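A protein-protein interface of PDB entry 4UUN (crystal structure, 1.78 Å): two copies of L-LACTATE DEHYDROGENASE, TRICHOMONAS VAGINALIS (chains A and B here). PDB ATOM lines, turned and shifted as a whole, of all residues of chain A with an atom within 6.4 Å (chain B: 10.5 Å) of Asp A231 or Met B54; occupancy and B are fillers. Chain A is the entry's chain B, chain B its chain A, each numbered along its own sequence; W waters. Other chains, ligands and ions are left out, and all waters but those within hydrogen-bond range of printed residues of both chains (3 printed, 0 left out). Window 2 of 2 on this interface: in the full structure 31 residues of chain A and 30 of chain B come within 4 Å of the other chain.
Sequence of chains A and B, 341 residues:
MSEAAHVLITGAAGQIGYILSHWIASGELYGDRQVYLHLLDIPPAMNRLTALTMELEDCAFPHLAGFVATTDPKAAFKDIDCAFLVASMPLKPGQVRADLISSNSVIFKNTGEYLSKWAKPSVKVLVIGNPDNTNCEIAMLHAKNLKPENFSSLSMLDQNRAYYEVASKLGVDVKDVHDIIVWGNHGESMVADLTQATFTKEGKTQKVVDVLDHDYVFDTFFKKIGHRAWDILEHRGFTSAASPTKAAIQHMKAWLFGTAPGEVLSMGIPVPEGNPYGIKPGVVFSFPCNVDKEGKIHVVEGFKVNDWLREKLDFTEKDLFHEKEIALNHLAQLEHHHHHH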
ATOM      1  N   HIS A 227     -15.410 -25.182   0.561  1.00  0.00           N
ATOM      2  CA  HIS A 227     -14.890 -23.950   1.150  1.00  0.00           C
ATOM      3  C   HIS A 227     -15.311 -22.726   0.347  1.00  0.00           C
ATOM      4  O   HIS A 227     -14.811 -21.620   0.566  1.00  0.00           O
ATOM      5  CB  HIS A 227     -13.364 -24.018   1.264  1.00  0.00           C
ATOM      6  CG  HIS A 227     -12.885 -25.036   2.253  1.00  0.00           C
ATOM      7  ND1 HIS A 227     -12.771 -26.376   1.948  1.00  0.00           N
ATOM      8  CD2 HIS A 227     -12.512 -24.912   3.548  1.00  0.00           C
ATOM      9  CE1 HIS A 227     -12.337 -27.032   3.009  1.00  0.00           C
ATOM     10  NE2 HIS A 227     -12.172 -26.167   3.994  1.00  0.00           N
ATOM     11  N   ARG A 228     -16.245 -22.927  -0.573  1.00  0.00           N
ATOM     12  CA  ARG A 228     -16.677 -21.868  -1.473  1.00  0.00           C
ATOM     13  C   ARG A 228     -17.448 -20.775  -0.738  1.00  0.00           C
ATOM     14  O   ARG A 228     -17.186 -19.582  -0.927  1.00  0.00           O
ATOM     15  CB  ARG A 228     -17.553 -22.460  -2.570  1.00  0.00           C
ATOM     16  CG  ARG A 228     -17.950 -21.477  -3.638  1.00  0.00           C
ATOM     17  CD  ARG A 228     -16.788 -21.094  -4.530  1.00  0.00           C
ATOM     18  NE  ARG A 228     -17.289 -20.366  -5.689  1.00  0.00           N
ATOM     19  CZ  ARG A 228     -16.542 -19.859  -6.661  1.00  0.00           C
ATOM     20  NH1 ARG A 228     -15.216 -19.973  -6.640  1.00  0.00           N
ATOM     21  NH2 ARG A 228     -17.136 -19.226  -7.662  1.00  0.00           N
ATOM     22  N   ALA A 229     -18.404 -21.194   0.084  1.00  0.00           N
ATOM     23  CA  ALA A 229     -19.230 -20.279   0.866  1.00  0.00           C
ATOM     24  C   ALA A 229     -18.372 -19.432   1.796  1.00  0.00           C
ATOM     25  O   ALA A 229     -18.622 -18.239   1.981  1.00  0.00           O
ATOM     26  CB  ALA A 229     -20.248 -21.063   1.672  1.00  0.00           C
ATOM     27  N   TRP A 230     -17.362 -20.063   2.388  1.00  0.00           N
ATOM     28  CA  TRP A 230     -16.474 -19.376   3.313  1.00  0.00           C
ATOM     29  C   TRP A 230     -15.661 -18.334   2.558  1.00  0.00           C
ATOM     30  O   TRP A 230     -15.437 -17.219   3.034  1.00  0.00           O
ATOM     31  CB  TRP A 230     -15.539 -20.380   3.988  1.00  0.00           C
ATOM     32  CG  TRP A 230     -14.562 -19.731   4.912  1.00  0.00           C
ATOM     33  CD1 TRP A 230     -14.786 -19.343   6.200  1.00  0.00           C
ATOM     34  CD2 TRP A 230     -13.202 -19.384   4.617  1.00  0.00           C
ATOM     35  NE1 TRP A 230     -13.651 -18.776   6.727  1.00  0.00           N
ATOM     36  CE2 TRP A 230     -12.665 -18.789   5.775  1.00  0.00           C
ATOM     37  CE3 TRP A 230     -12.388 -19.519   3.487  1.00  0.00           C
ATOM     38  CZ2 TRP A 230     -11.351 -18.332   5.838  1.00  0.00           C
ATOM     39  CZ3 TRP A 230     -11.083 -19.062   3.551  1.00  0.00           C
ATOM     40  CH2 TRP A 230     -10.578 -18.476   4.718  1.00  0.00           C
ATOM     41  N   ASP A 231     -15.227 -18.717   1.367  1.00  0.00           N
ATOM     42  CA  ASP A 231     -14.416 -17.864   0.525  1.00  0.00           C
ATOM     43  C   ASP A 231     -15.213 -16.615   0.104  1.00  0.00           C
ATOM     44  O   ASP A 231     -14.662 -15.513   0.029  1.00  0.00           O
ATOM     45  CB  ASP A 231     -13.940 -18.680  -0.681  1.00  0.00           C
ATOM     46  CG  ASP A 231     -12.569 -18.277  -1.159  1.00  0.00           C
ATOM     47  OD1 ASP A 231     -12.121 -17.161  -0.829  1.00  0.00           O
ATOM     48  OD2 ASP A 231     -11.936 -19.084  -1.874  1.00  0.00           O
ATOM     49  N   ILE A 232     -16.504 -16.785  -0.149  1.00  0.00           N
ATOM     50  CA  ILE A 232     -17.364 -15.653  -0.486  1.00  0.00           C
ATOM     51  C   ILE A 232     -17.517 -14.720   0.725  1.00  0.00           C
ATOM     52  O   ILE A 232     -17.384 -13.503   0.606  1.00  0.00           O
ATOM     53  CB  ILE A 232     -18.730 -16.146  -0.998  1.00  0.00           C
ATOM     54  CG1 ILE A 232     -18.568 -16.710  -2.413  1.00  0.00           C
ATOM     55  CG2 ILE A 232     -19.758 -15.024  -1.020  1.00  0.00           C
ATOM     56  CD1 ILE A 232     -19.749 -17.509  -2.898  1.00  0.00           C
ATOM     57  N   LEU A 233     -17.796 -15.304   1.884  1.00  0.00           N
ATOM     58  CA  LEU A 233     -17.913 -14.537   3.120  1.00  0.00           C
ATOM     59  C   LEU A 233     -16.628 -13.773   3.410  1.00  0.00           C
ATOM     60  O   LEU A 233     -16.658 -12.615   3.823  1.00  0.00           O
ATOM     61  CB  LEU A 233     -18.219 -15.485   4.276  1.00  0.00           C
ATOM     62  CG  LEU A 233     -18.283 -14.854   5.663  1.00  0.00           C
ATOM     63  CD1 LEU A 233     -19.353 -13.769   5.709  1.00  0.00           C
ATOM     64  CD2 LEU A 233     -18.545 -15.934   6.691  1.00  0.00           C
ATOM     65  N   GLU A 234     -15.503 -14.436   3.177  1.00  0.00           N
ATOM     66  CA  GLU A 234     -14.193 -13.836   3.347  1.00  0.00           C
ATOM     67  C   GLU A 234     -14.070 -12.534   2.560  1.00  0.00           C
ATOM     68  O   GLU A 234     -13.629 -11.522   3.096  1.00  0.00           O
ATOM     69  CB  GLU A 234     -13.119 -14.810   2.870  1.00  0.00           C
ATOM     70  CG  GLU A 234     -11.713 -14.441   3.288  1.00  0.00           C
ATOM     71  CD  GLU A 234     -11.397 -14.849   4.716  1.00  0.00           C
ATOM     72  OE1 GLU A 234     -12.326 -15.254   5.446  1.00  0.00           O
ATOM     73  OE2 GLU A 234     -10.214 -14.763   5.106  1.00  0.00           O
ATOM     74  N   HIS A 235     -14.460 -12.570   1.286  1.00  0.00           N
ATOM     75  CA  HIS A 235     -14.295 -11.423   0.393  1.00  0.00           C
ATOM     76  C   HIS A 235     -15.465 -10.435   0.484  1.00  0.00           C
ATOM     77  O   HIS A 235     -15.281  -9.231   0.313  1.00  0.00           O
ATOM     78  CB  HIS A 235     -14.156 -11.891  -1.059  1.00  0.00           C
ATOM     79  CG  HIS A 235     -12.865 -12.589  -1.365  1.00  0.00           C
ATOM     80  ND1 HIS A 235     -12.639 -13.911  -1.050  1.00  0.00           N
ATOM     81  CD2 HIS A 235     -11.740 -12.153  -1.980  1.00  0.00           C
ATOM     82  CE1 HIS A 235     -11.428 -14.257  -1.451  1.00  0.00           C
ATOM     83  NE2 HIS A 235     -10.861 -13.207  -2.018  1.00  0.00           N
ATOM     84  N   ARG A 236     -16.665 -10.953   0.734  1.00  0.00           N
ATOM     85  CA  ARG A 236     -17.889 -10.146   0.698  1.00  0.00           C
ATOM     86  C   ARG A 236     -18.140  -9.447   2.029  1.00  0.00           C
ATOM     87  O   ARG A 236     -18.571  -8.292   2.063  1.00  0.00           O
ATOM     88  CB  ARG A 236     -19.088 -11.036   0.348  1.00  0.00           C
ATOM     89  CG  ARG A 236     -20.456 -10.351   0.350  1.00  0.00           C
ATOM     90  CD  ARG A 236     -21.512 -11.292  -0.223  1.00  0.00           C
ATOM     91  NE  ARG A 236     -22.886 -10.957   0.157  1.00  0.00           N
ATOM     92  CZ  ARG A 236     -23.614  -9.999  -0.410  1.00  0.00           C
ATOM     93  NH1 ARG A 236     -23.102  -9.248  -1.376  1.00  0.00           N
ATOM     94  NH2 ARG A 236     -24.855  -9.781   0.000  1.00  0.00           N
ATOM     95  N   SER A 243     -27.006 -16.007  -5.148  1.00  0.00           N
ATOM     96  CA  SER A 243     -26.856 -17.359  -5.695  1.00  0.00           C
ATOM     97  C   SER A 243     -27.781 -18.409  -5.034  1.00  0.00           C
ATOM     98  O   SER A 243     -28.321 -19.267  -5.727  1.00  0.00           O
ATOM     99  CB  SER A 243     -25.382 -17.812  -5.728  1.00  0.00           C
ATOM    100  OG  SER A 243     -24.737 -17.704  -4.474  1.00  0.00           O
ATOM    101  N   TYR B  18     -24.598  -5.414  -7.682  1.00  0.00           N
ATOM    102  CA  TYR B  18     -24.764  -6.800  -7.233  1.00  0.00           C
ATOM    103  C   TYR B  18     -26.013  -7.442  -7.825  1.00  0.00           C
ATOM    104  O   TYR B  18     -25.959  -8.544  -8.373  1.00  0.00           O
ATOM    105  CB  TYR B  18     -24.851  -6.818  -5.706  1.00  0.00           C
ATOM    106  CG  TYR B  18     -25.002  -8.177  -5.060  1.00  0.00           C
ATOM    107  CD1 TYR B  18     -23.914  -9.032  -4.920  1.00  0.00           C
ATOM    108  CD2 TYR B  18     -26.226  -8.594  -4.558  1.00  0.00           C
ATOM    109  CE1 TYR B  18     -24.047 -10.264  -4.311  1.00  0.00           C
ATOM    110  CE2 TYR B  18     -26.370  -9.834  -3.945  1.00  0.00           C
ATOM    111  CZ  TYR B  18     -25.277 -10.665  -3.827  1.00  0.00           C
ATOM    112  OH  TYR B  18     -25.404 -11.894  -3.211  1.00  0.00           O
ATOM    113  N   SER B  21     -26.153  -7.142 -12.021  1.00  0.00           N
ATOM    114  CA  SER B  21     -25.332  -8.131 -12.709  1.00  0.00           C
ATOM    115  C   SER B  21     -26.032  -9.496 -12.752  1.00  0.00           C
ATOM    116  O   SER B  21     -26.099 -10.125 -13.813  1.00  0.00           O
ATOM    117  CB  SER B  21     -23.938  -8.226 -12.071  1.00  0.00           C
ATOM    118  OG  SER B  21     -24.009  -8.561 -10.698  1.00  0.00           O
ATOM    119  N   HIS B  22     -26.574  -9.940 -11.622  1.00  0.00           N
ATOM    120  CA  HIS B  22     -27.274 -11.217 -11.571  1.00  0.00           C
ATOM    121  C   HIS B  22     -28.533 -11.248 -12.454  1.00  0.00           C
ATOM    122  O   HIS B  22     -28.776 -12.223 -13.158  1.00  0.00           O
ATOM    123  CB  HIS B  22     -27.647 -11.569 -10.121  1.00  0.00           C
ATOM    124  CG  HIS B  22     -26.519 -12.160  -9.334  1.00  0.00           C
ATOM    125  ND1 HIS B  22     -25.638 -11.393  -8.599  1.00  0.00           N
ATOM    126  CD2 HIS B  22     -26.128 -13.445  -9.163  1.00  0.00           C
ATOM    127  CE1 HIS B  22     -24.751 -12.179  -8.016  1.00  0.00           C
ATOM    128  NE2 HIS B  22     -25.025 -13.431  -8.343  1.00  0.00           N
ATOM    129  N   LEU B  37     -20.361  -9.814 -19.154  1.00  0.00           N
ATOM    130  CA  LEU B  37     -20.374  -8.669 -18.255  1.00  0.00           C
ATOM    131  C   LEU B  37     -18.997  -8.036 -18.104  1.00  0.00           C
ATOM    132  O   LEU B  37     -18.006  -8.726 -17.892  1.00  0.00           O
ATOM    133  CB  LEU B  37     -20.900  -9.079 -16.880  1.00  0.00           C
ATOM    134  CG  LEU B  37     -22.334  -9.610 -16.855  1.00  0.00           C
ATOM    135  CD1 LEU B  37     -22.693 -10.103 -15.464  1.00  0.00           C
ATOM    136  CD2 LEU B  37     -23.314  -8.545 -17.319  1.00  0.00           C
ATOM    137  N   LEU B  39     -17.393  -5.637 -15.497  1.00  0.00           N
ATOM    138  CA  LEU B  39     -17.673  -5.179 -14.145  1.00  0.00           C
ATOM    139  C   LEU B  39     -16.540  -4.287 -13.655  1.00  0.00           C
ATOM    140  O   LEU B  39     -15.436  -4.768 -13.394  1.00  0.00           O
ATOM    141  CB  LEU B  39     -17.845  -6.389 -13.230  1.00  0.00           C
ATOM    142  CG  LEU B  39     -18.880  -7.418 -13.710  1.00  0.00           C
ATOM    143  CD1 LEU B  39     -18.862  -8.665 -12.822  1.00  0.00           C
ATOM    144  CD2 LEU B  39     -20.284  -6.817 -13.758  1.00  0.00           C
ATOM    145  N   MET B  46     -12.042  -4.146  -4.721  1.00  0.00           N
ATOM    146  CA  MET B  46     -11.611  -5.338  -5.453  1.00  0.00           C
ATOM    147  C   MET B  46     -12.128  -6.632  -4.822  1.00  0.00           C
ATOM    148  O   MET B  46     -12.617  -7.514  -5.523  1.00  0.00           O
ATOM    149  CB  MET B  46     -10.078  -5.384  -5.569  1.00  0.00           C
ATOM    150  CG  MET B  46      -9.500  -4.489  -6.672  1.00  0.00           C
ATOM    151  SD  MET B  46      -7.698  -4.586  -6.859  1.00  0.00           S
ATOM    152  CE  MET B  46      -7.499  -6.125  -7.758  1.00  0.00           C
ATOM    153  N   ASN B  47     -12.026  -6.740  -3.499  1.00  0.00           N
ATOM    154  CA  ASN B  47     -12.451  -7.948  -2.793  1.00  0.00           C
ATOM    155  C   ASN B  47     -13.958  -8.163  -2.924  1.00  0.00           C
ATOM    156  O   ASN B  47     -14.410  -9.285  -3.167  1.00  0.00           O
ATOM    157  CB  ASN B  47     -12.033  -7.911  -1.323  1.00  0.00           C
ATOM    158  CG  ASN B  47     -10.550  -8.171  -1.135  1.00  0.00           C
ATOM    159  OD1 ASN B  47      -9.904  -8.804  -1.977  1.00  0.00           O
ATOM    160  ND2 ASN B  47     -10.001  -7.688  -0.027  1.00  0.00           N
ATOM    161  N   ARG B  48     -14.737  -7.093  -2.787  1.00  0.00           N
ATOM    162  CA  ARG B  48     -16.181  -7.190  -2.977  1.00  0.00           C
ATOM    163  C   ARG B  48     -16.519  -7.545  -4.419  1.00  0.00           C
ATOM    164  O   ARG B  48     -17.505  -8.233  -4.685  1.00  0.00           O
ATOM    165  CB  ARG B  48     -16.882  -5.886  -2.595  1.00  0.00           C
ATOM    166  CG  ARG B  48     -16.981  -5.655  -1.102  1.00  0.00           C
ATOM    167  CD  ARG B  48     -18.229  -4.866  -0.724  1.00  0.00           C
ATOM    168  NE  ARG B  48     -18.501  -3.745  -1.624  1.00  0.00           N
ATOM    169  CZ  ARG B  48     -17.839  -2.588  -1.619  1.00  0.00           C
ATOM    170  NH1 ARG B  48     -16.834  -2.384  -0.772  1.00  0.00           N
ATOM    171  NH2 ARG B  48     -18.180  -1.633  -2.477  1.00  0.00           N
ATOM    172  N   LEU B  49     -15.706  -7.066  -5.350  1.00  0.00           N
ATOM    173  CA  LEU B  49     -15.907  -7.380  -6.755  1.00  0.00           C
ATOM    174  C   LEU B  49     -15.625  -8.867  -6.998  1.00  0.00           C
ATOM    175  O   LEU B  49     -16.364  -9.546  -7.712  1.00  0.00           O
ATOM    176  CB  LEU B  49     -15.007  -6.508  -7.627  1.00  0.00           C
ATOM    177  CG  LEU B  49     -15.257  -6.565  -9.136  1.00  0.00           C
ATOM    178  CD1 LEU B  49     -16.701  -6.228  -9.471  1.00  0.00           C
ATOM    179  CD2 LEU B  49     -14.330  -5.620  -9.862  1.00  0.00           C
ATOM    180  N   THR B  50     -14.554  -9.366  -6.392  1.00  0.00           N
ATOM    181  CA  THR B  50     -14.216 -10.787  -6.469  1.00  0.00           C
ATOM    182  C   THR B  50     -15.355 -11.647  -5.928  1.00  0.00           C
ATOM    183  O   THR B  50     -15.729 -12.649  -6.534  1.00  0.00           O
ATOM    184  CB  THR B  50     -12.933 -11.085  -5.683  1.00  0.00           C
ATOM    185  OG1 THR B  50     -11.835 -10.394  -6.288  1.00  0.00           O
ATOM    186  CG2 THR B  50     -12.638 -12.586  -5.656  1.00  0.00           C
ATOM    187  N   ALA B  51     -15.912 -11.241  -4.792  1.00  0.00           N
ATOM    188  CA  ALA B  51     -17.036 -11.943  -4.184  1.00  0.00           C
ATOM    189  C   ALA B  51     -18.235 -12.006  -5.128  1.00  0.00           C
ATOM    190  O   ALA B  51     -18.881 -13.041  -5.258  1.00  0.00           O
ATOM    191  CB  ALA B  51     -17.441 -11.266  -2.893  1.00  0.00           C
ATOM    192  N   LEU B  52     -18.530 -10.883  -5.775  1.00  0.00           N
ATOM    193  CA  LEU B  52     -19.593 -10.832  -6.767  1.00  0.00           C
ATOM    194  C   LEU B  52     -19.375 -11.841  -7.894  1.00  0.00           C
ATOM    195  O   LEU B  52     -20.304 -12.549  -8.283  1.00  0.00           O
ATOM    196  CB  LEU B  52     -19.711  -9.421  -7.350  1.00  0.00           C
ATOM    197  CG  LEU B  52     -20.575  -9.309  -8.613  1.00  0.00           C
ATOM    198  CD1 LEU B  52     -21.985  -9.798  -8.347  1.00  0.00           C
ATOM    199  CD2 LEU B  52     -20.583  -7.871  -9.113  1.00  0.00           C
ATOM    200  N   THR B  53     -18.162 -11.897  -8.434  1.00  0.00           N
ATOM    201  CA  THR B  53     -17.888 -12.834  -9.525  1.00  0.00           C
ATOM    202  C   THR B  53     -18.077 -14.294  -9.091  1.00  0.00           C
ATOM    203  O   THR B  53     -18.545 -15.111  -9.869  1.00  0.00           O
ATOM    204  CB  THR B  53     -16.478 -12.661 -10.155  1.00  0.00           C
ATOM    205  OG1 THR B  53     -15.449 -13.015  -9.217  1.00  0.00           O
ATOM    206  CG2 THR B  53     -16.265 -11.230 -10.659  1.00  0.00           C
ATOM    207  N   MET B  54     -17.716 -14.607  -7.851  1.00  0.00           N
ATOM    208  CA  MET B  54     -17.847 -15.969  -7.342  1.00  0.00           C
ATOM    209  C   MET B  54     -19.314 -16.385  -7.274  1.00  0.00           C
ATOM    210  O   MET B  54     -19.664 -17.523  -7.598  1.00  0.00           O
ATOM    211  CB  MET B  54     -17.207 -16.078  -5.958  1.00  0.00           C
ATOM    212  CG  MET B  54     -15.715 -15.836  -5.943  1.00  0.00           C
ATOM    213  SD  MET B  54     -15.085 -15.526  -4.279  1.00  0.00           S
ATOM    214  CE  MET B  54     -15.331 -17.128  -3.537  1.00  0.00           C
ATOM    215  N   GLU B  55     -20.177 -15.465  -6.855  1.00  0.00           N
ATOM    216  CA  GLU B  55     -21.605 -15.759  -6.811  1.00  0.00           C
ATOM    217  C   GLU B  55     -22.196 -15.892  -8.212  1.00  0.00           C
ATOM    218  O   GLU B  55     -23.015 -16.784  -8.442  1.00  0.00           O
ATOM    219  CB  GLU B  55     -22.374 -14.733  -5.985  1.00  0.00           C
ATOM    220  CG  GLU B  55     -22.461 -15.117  -4.522  1.00  0.00           C
ATOM    221  CD  GLU B  55     -23.567 -14.405  -3.793  1.00  0.00           C
ATOM    222  OE1 GLU B  55     -23.326 -13.286  -3.299  1.00  0.00           O
ATOM    223  OE2 GLU B  55     -24.674 -14.969  -3.711  1.00  0.00           O
ATOM    224  N   LEU B  56     -21.791 -15.022  -9.144  1.00  0.00           N
ATOM    225  CA  LEU B  56     -22.236 -15.145 -10.532  1.00  0.00           C
ATOM    226  C   LEU B  56     -21.883 -16.530 -11.065  1.00  0.00           C
ATOM    227  O   LEU B  56     -22.714 -17.206 -11.671  1.00  0.00           O
ATOM    228  CB  LEU B  56     -21.602 -14.071 -11.415  1.00  0.00           C
ATOM    229  CG  LEU B  56     -22.078 -12.641 -11.154  1.00  0.00           C
ATOM    230  CD1 LEU B  56     -21.230 -11.648 -11.940  1.00  0.00           C
ATOM    231  CD2 LEU B  56     -23.544 -12.490 -11.522  1.00  0.00           C
ATOM    232  N   GLU B  57     -20.643 -16.941 -10.816  1.00  0.00           N
ATOM    233  CA  GLU B  57     -20.169 -18.267 -11.195  1.00  0.00           C
ATOM    234  C   GLU B  57     -21.057 -19.352 -10.587  1.00  0.00           C
ATOM    235  O   GLU B  57     -21.459 -20.295 -11.275  1.00  0.00           O
ATOM    236  CB  GLU B  57     -18.719 -18.449 -10.741  1.00  0.00           C
ATOM    237  CG  GLU B  57     -17.703 -17.675 -11.577  1.00  0.00           C
ATOM    238  CD  GLU B  57     -16.279 -17.786 -11.047  1.00  0.00           C
ATOM    239  OE1 GLU B  57     -16.086 -18.297  -9.924  1.00  0.00           O
ATOM    240  OE2 GLU B  57     -15.351 -17.367 -11.765  1.00  0.00           O
ATOM    241  N   ASP B  58     -21.374 -19.200  -9.306  1.00  0.00           N
ATOM    242  CA  ASP B  58     -22.136 -20.208  -8.561  1.00  0.00           C
ATOM    243  C   ASP B  58     -23.621 -20.307  -8.952  1.00  0.00           C
ATOM    244  O   ASP B  58     -24.347 -21.156  -8.432  1.00  0.00           O
ATOM    245  CB  ASP B  58     -22.029 -19.937  -7.054  1.00  0.00           C
ATOM    246  CG  ASP B  58     -20.645 -20.231  -6.495  1.00  0.00           C
ATOM    247  OD1 ASP B  58     -19.774 -20.737  -7.245  1.00  0.00           O
ATOM    248  OD2 ASP B  58     -20.440 -19.978  -5.284  1.00  0.00           O
ATOM    249  N   CYS B  59     -24.081 -19.437  -9.845  1.00  0.00           N
ATOM    250  CA  CYS B  59     -25.427 -19.555 -10.399  1.00  0.00           C
ATOM    251  C   CYS B  59     -25.511 -20.487 -11.616  1.00  0.00           C
ATOM    252  O   CYS B  59     -26.606 -20.896 -12.026  1.00  0.00           O
ATOM    253  CB  CYS B  59     -25.970 -18.177 -10.780  1.00  0.00           C
ATOM    254  SG  CYS B  59     -26.305 -17.118  -9.352  1.00  0.00           S
ATOM    255  N   ALA B  60     -24.362 -20.803 -12.201  1.00  0.00           N
ATOM    256  CA  ALA B  60     -24.312 -21.580 -13.437  1.00  0.00           C
ATOM    257  C   ALA B  60     -25.302 -21.067 -14.491  1.00  0.00           C
ATOM    258  O   ALA B  60     -26.064 -21.845 -15.069  1.00  0.00           O
ATOM    259  CB  ALA B  60     -24.554 -23.061 -13.136  1.00  0.00           C
ATOM    260  N   PHE B  61     -25.289 -19.754 -14.725  1.00  0.00           N
ATOM    261  CA  PHE B  61     -26.167 -19.110 -15.703  1.00  0.00           C
ATOM    262  C   PHE B  61     -25.833 -19.537 -17.134  1.00  0.00           C
ATOM    263  O   PHE B  61     -24.735 -19.274 -17.606  1.00  0.00           O
ATOM    264  CB  PHE B  61     -25.997 -17.585 -15.665  1.00  0.00           C
ATOM    265  CG  PHE B  61     -26.615 -16.897 -14.469  1.00  0.00           C
ATOM    266  CD1 PHE B  61     -27.968 -16.980 -14.212  1.00  0.00           C
ATOM    267  CD2 PHE B  61     -25.837 -16.095 -13.651  1.00  0.00           C
ATOM    268  CE1 PHE B  61     -28.523 -16.319 -13.130  1.00  0.00           C
ATOM    269  CE2 PHE B  61     -26.389 -15.429 -12.573  1.00  0.00           C
ATOM    270  CZ  PHE B  61     -27.730 -15.537 -12.318  1.00  0.00           C
ATOM    271  N   LEU B  64     -24.651 -16.551 -19.339  1.00  0.00           N
ATOM    272  CA  LEU B  64     -23.392 -15.853 -19.059  1.00  0.00           C
ATOM    273  C   LEU B  64     -22.235 -16.453 -19.854  1.00  0.00           C
ATOM    274  O   LEU B  64     -21.753 -17.544 -19.542  1.00  0.00           O
ATOM    275  CB  LEU B  64     -23.075 -15.879 -17.560  1.00  0.00           C
ATOM    276  CG  LEU B  64     -21.895 -15.032 -17.070  1.00  0.00           C
ATOM    277  CD1 LEU B  64     -22.075 -13.552 -17.403  1.00  0.00           C
ATOM    278  CD2 LEU B  64     -21.696 -15.208 -15.574  1.00  0.00           C
ATOM    279  N   PHE B  67     -17.024 -12.920 -18.194  1.00  0.00           N
ATOM    280  CA  PHE B  67     -16.981 -11.594 -17.604  1.00  0.00           C
ATOM    281  C   PHE B  67     -15.575 -11.067 -17.420  1.00  0.00           C
ATOM    282  O   PHE B  67     -14.612 -11.828 -17.331  1.00  0.00           O
ATOM    283  CB  PHE B  67     -17.705 -11.562 -16.251  1.00  0.00           C
ATOM    284  CG  PHE B  67     -17.168 -12.547 -15.243  1.00  0.00           C
ATOM    285  CD1 PHE B  67     -16.085 -12.227 -14.444  1.00  0.00           C
ATOM    286  CD2 PHE B  67     -17.761 -13.788 -15.089  1.00  0.00           C
ATOM    287  CE1 PHE B  67     -15.592 -13.135 -13.519  1.00  0.00           C
ATOM    288  CE2 PHE B  67     -17.273 -14.700 -14.170  1.00  0.00           C
ATOM    289  CZ  PHE B  67     -16.189 -14.374 -13.382  1.00  0.00           C
ATOM    290  N   ALA B  69     -13.721  -8.429 -14.679  1.00  0.00           N
ATOM    291  CA  ALA B  69     -13.921  -7.770 -13.394  1.00  0.00           C
ATOM    292  C   ALA B  69     -12.613  -7.110 -13.015  1.00  0.00           C
ATOM    293  O   ALA B  69     -11.616  -7.791 -12.750  1.00  0.00           O
ATOM    294  CB  ALA B  69     -14.355  -8.772 -12.340  1.00  0.00           C
HETATM  295  O   HOH W   1     -27.120 -21.161  -7.648  1.00  0.00           O
HETATM  296  O   HOH W   2     -13.798 -18.698  -8.686  1.00  0.00           O
HETATM  297  O   HOH W   3     -22.425 -19.059  -3.725  1.00  0.00           O
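NH2 of Arg A228 is in hydrogen-bond range of O of Met B54.
The side-chain carboxylate (OE2) of Glu B55 lies within hydrogen-bond range of the side-chain hydroxyl (OG) of Ser A243, at 2.8 Å.
OE1 of Glu B57 lies within salt-bridge range of NH2 of Arg A228.
OD1 of Asp B58 lies within salt-bridge range of NE of Arg A228, at 3.0 Å.
O of Tyr B18 is in hydrogen-bond range of OG of Ser B21, 3.0 Å away.
A ring nitrogen (ND1) of His B22 is in hydrogen-bond range of the backbone carbonyl oxygen (O) of Tyr B18 (2.9 Å).
The side-chain hydroxyl (OH) of Tyr B18 lies within hydrogen-bond range of the side-chain carboxylate (OE1) of Glu B55.
The backbone carbonyl oxygen (O) of Thr B50 sits at hydrogen-bond distance from the side-chain hydroxyl (OG1) of Thr B53 (2.7 Å).
O of Glu B55 is in hydrogen-bond range of SG of Cys B59 (3.4 Å).
O of Asp A231 sits at hydrogen-bond distance from ND1 of His A235.
Asp A231 touches Met B54 (CB to CE, 3.5 Å).
CG1 of Ile A232 touches CE of Met B54, 3.5 Å away.
CD1 of Ile A232 touches CG of Glu B55, 3.96 Å away.
Asp B58 touches Ile A232 (OD2 to CD1, 3.5 Å).
His A235 touches Asn B47 (CB to O, 3.4 Å).
O of His A235 touches N of Arg B48, at 3.8 Å.
His A235 touches Thr B50.
His A235 touches Ala B51 (CB to CB, 3.8 Å).
Arg A236 touches Tyr B18.
CB of Ala B51 touches CB of Arg A236, 3.6 Å away.
Printed residues of chain B within 4 Å of Asp A231: Met B54.
No residue of chain B comes within 4 Å of Ala A229.
Of the printed residues of chain B, Ile A232 touches Met B54 (3.5 Å), Glu B55 (3.96 Å) and Asp B58 (3.5 Å).
Printed residues of chain A within 4 Å of Glu B55: Ile A232 and Ser A243.
Hydrophobic or aromatic side chains of chain A within 4 Å of the printed part of chain B: Ile A232 and His A235.
Among the printed residues, 15 pairs touch across the chains.
No position is printed for both chains.
Water W2 bridges the side-chain carboxylate of Glu B57 (2.6 Å) and the guanidinium group of Arg A228 (2.8 Å).
Water W3 bridges the side-chain carboxylate of Asp B58 (2.7 Å) and the side-chain hydroxyl of Ser A243 (2.8 Å).
Water W1 bridges O of Asp B58 and O of Ser A243.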
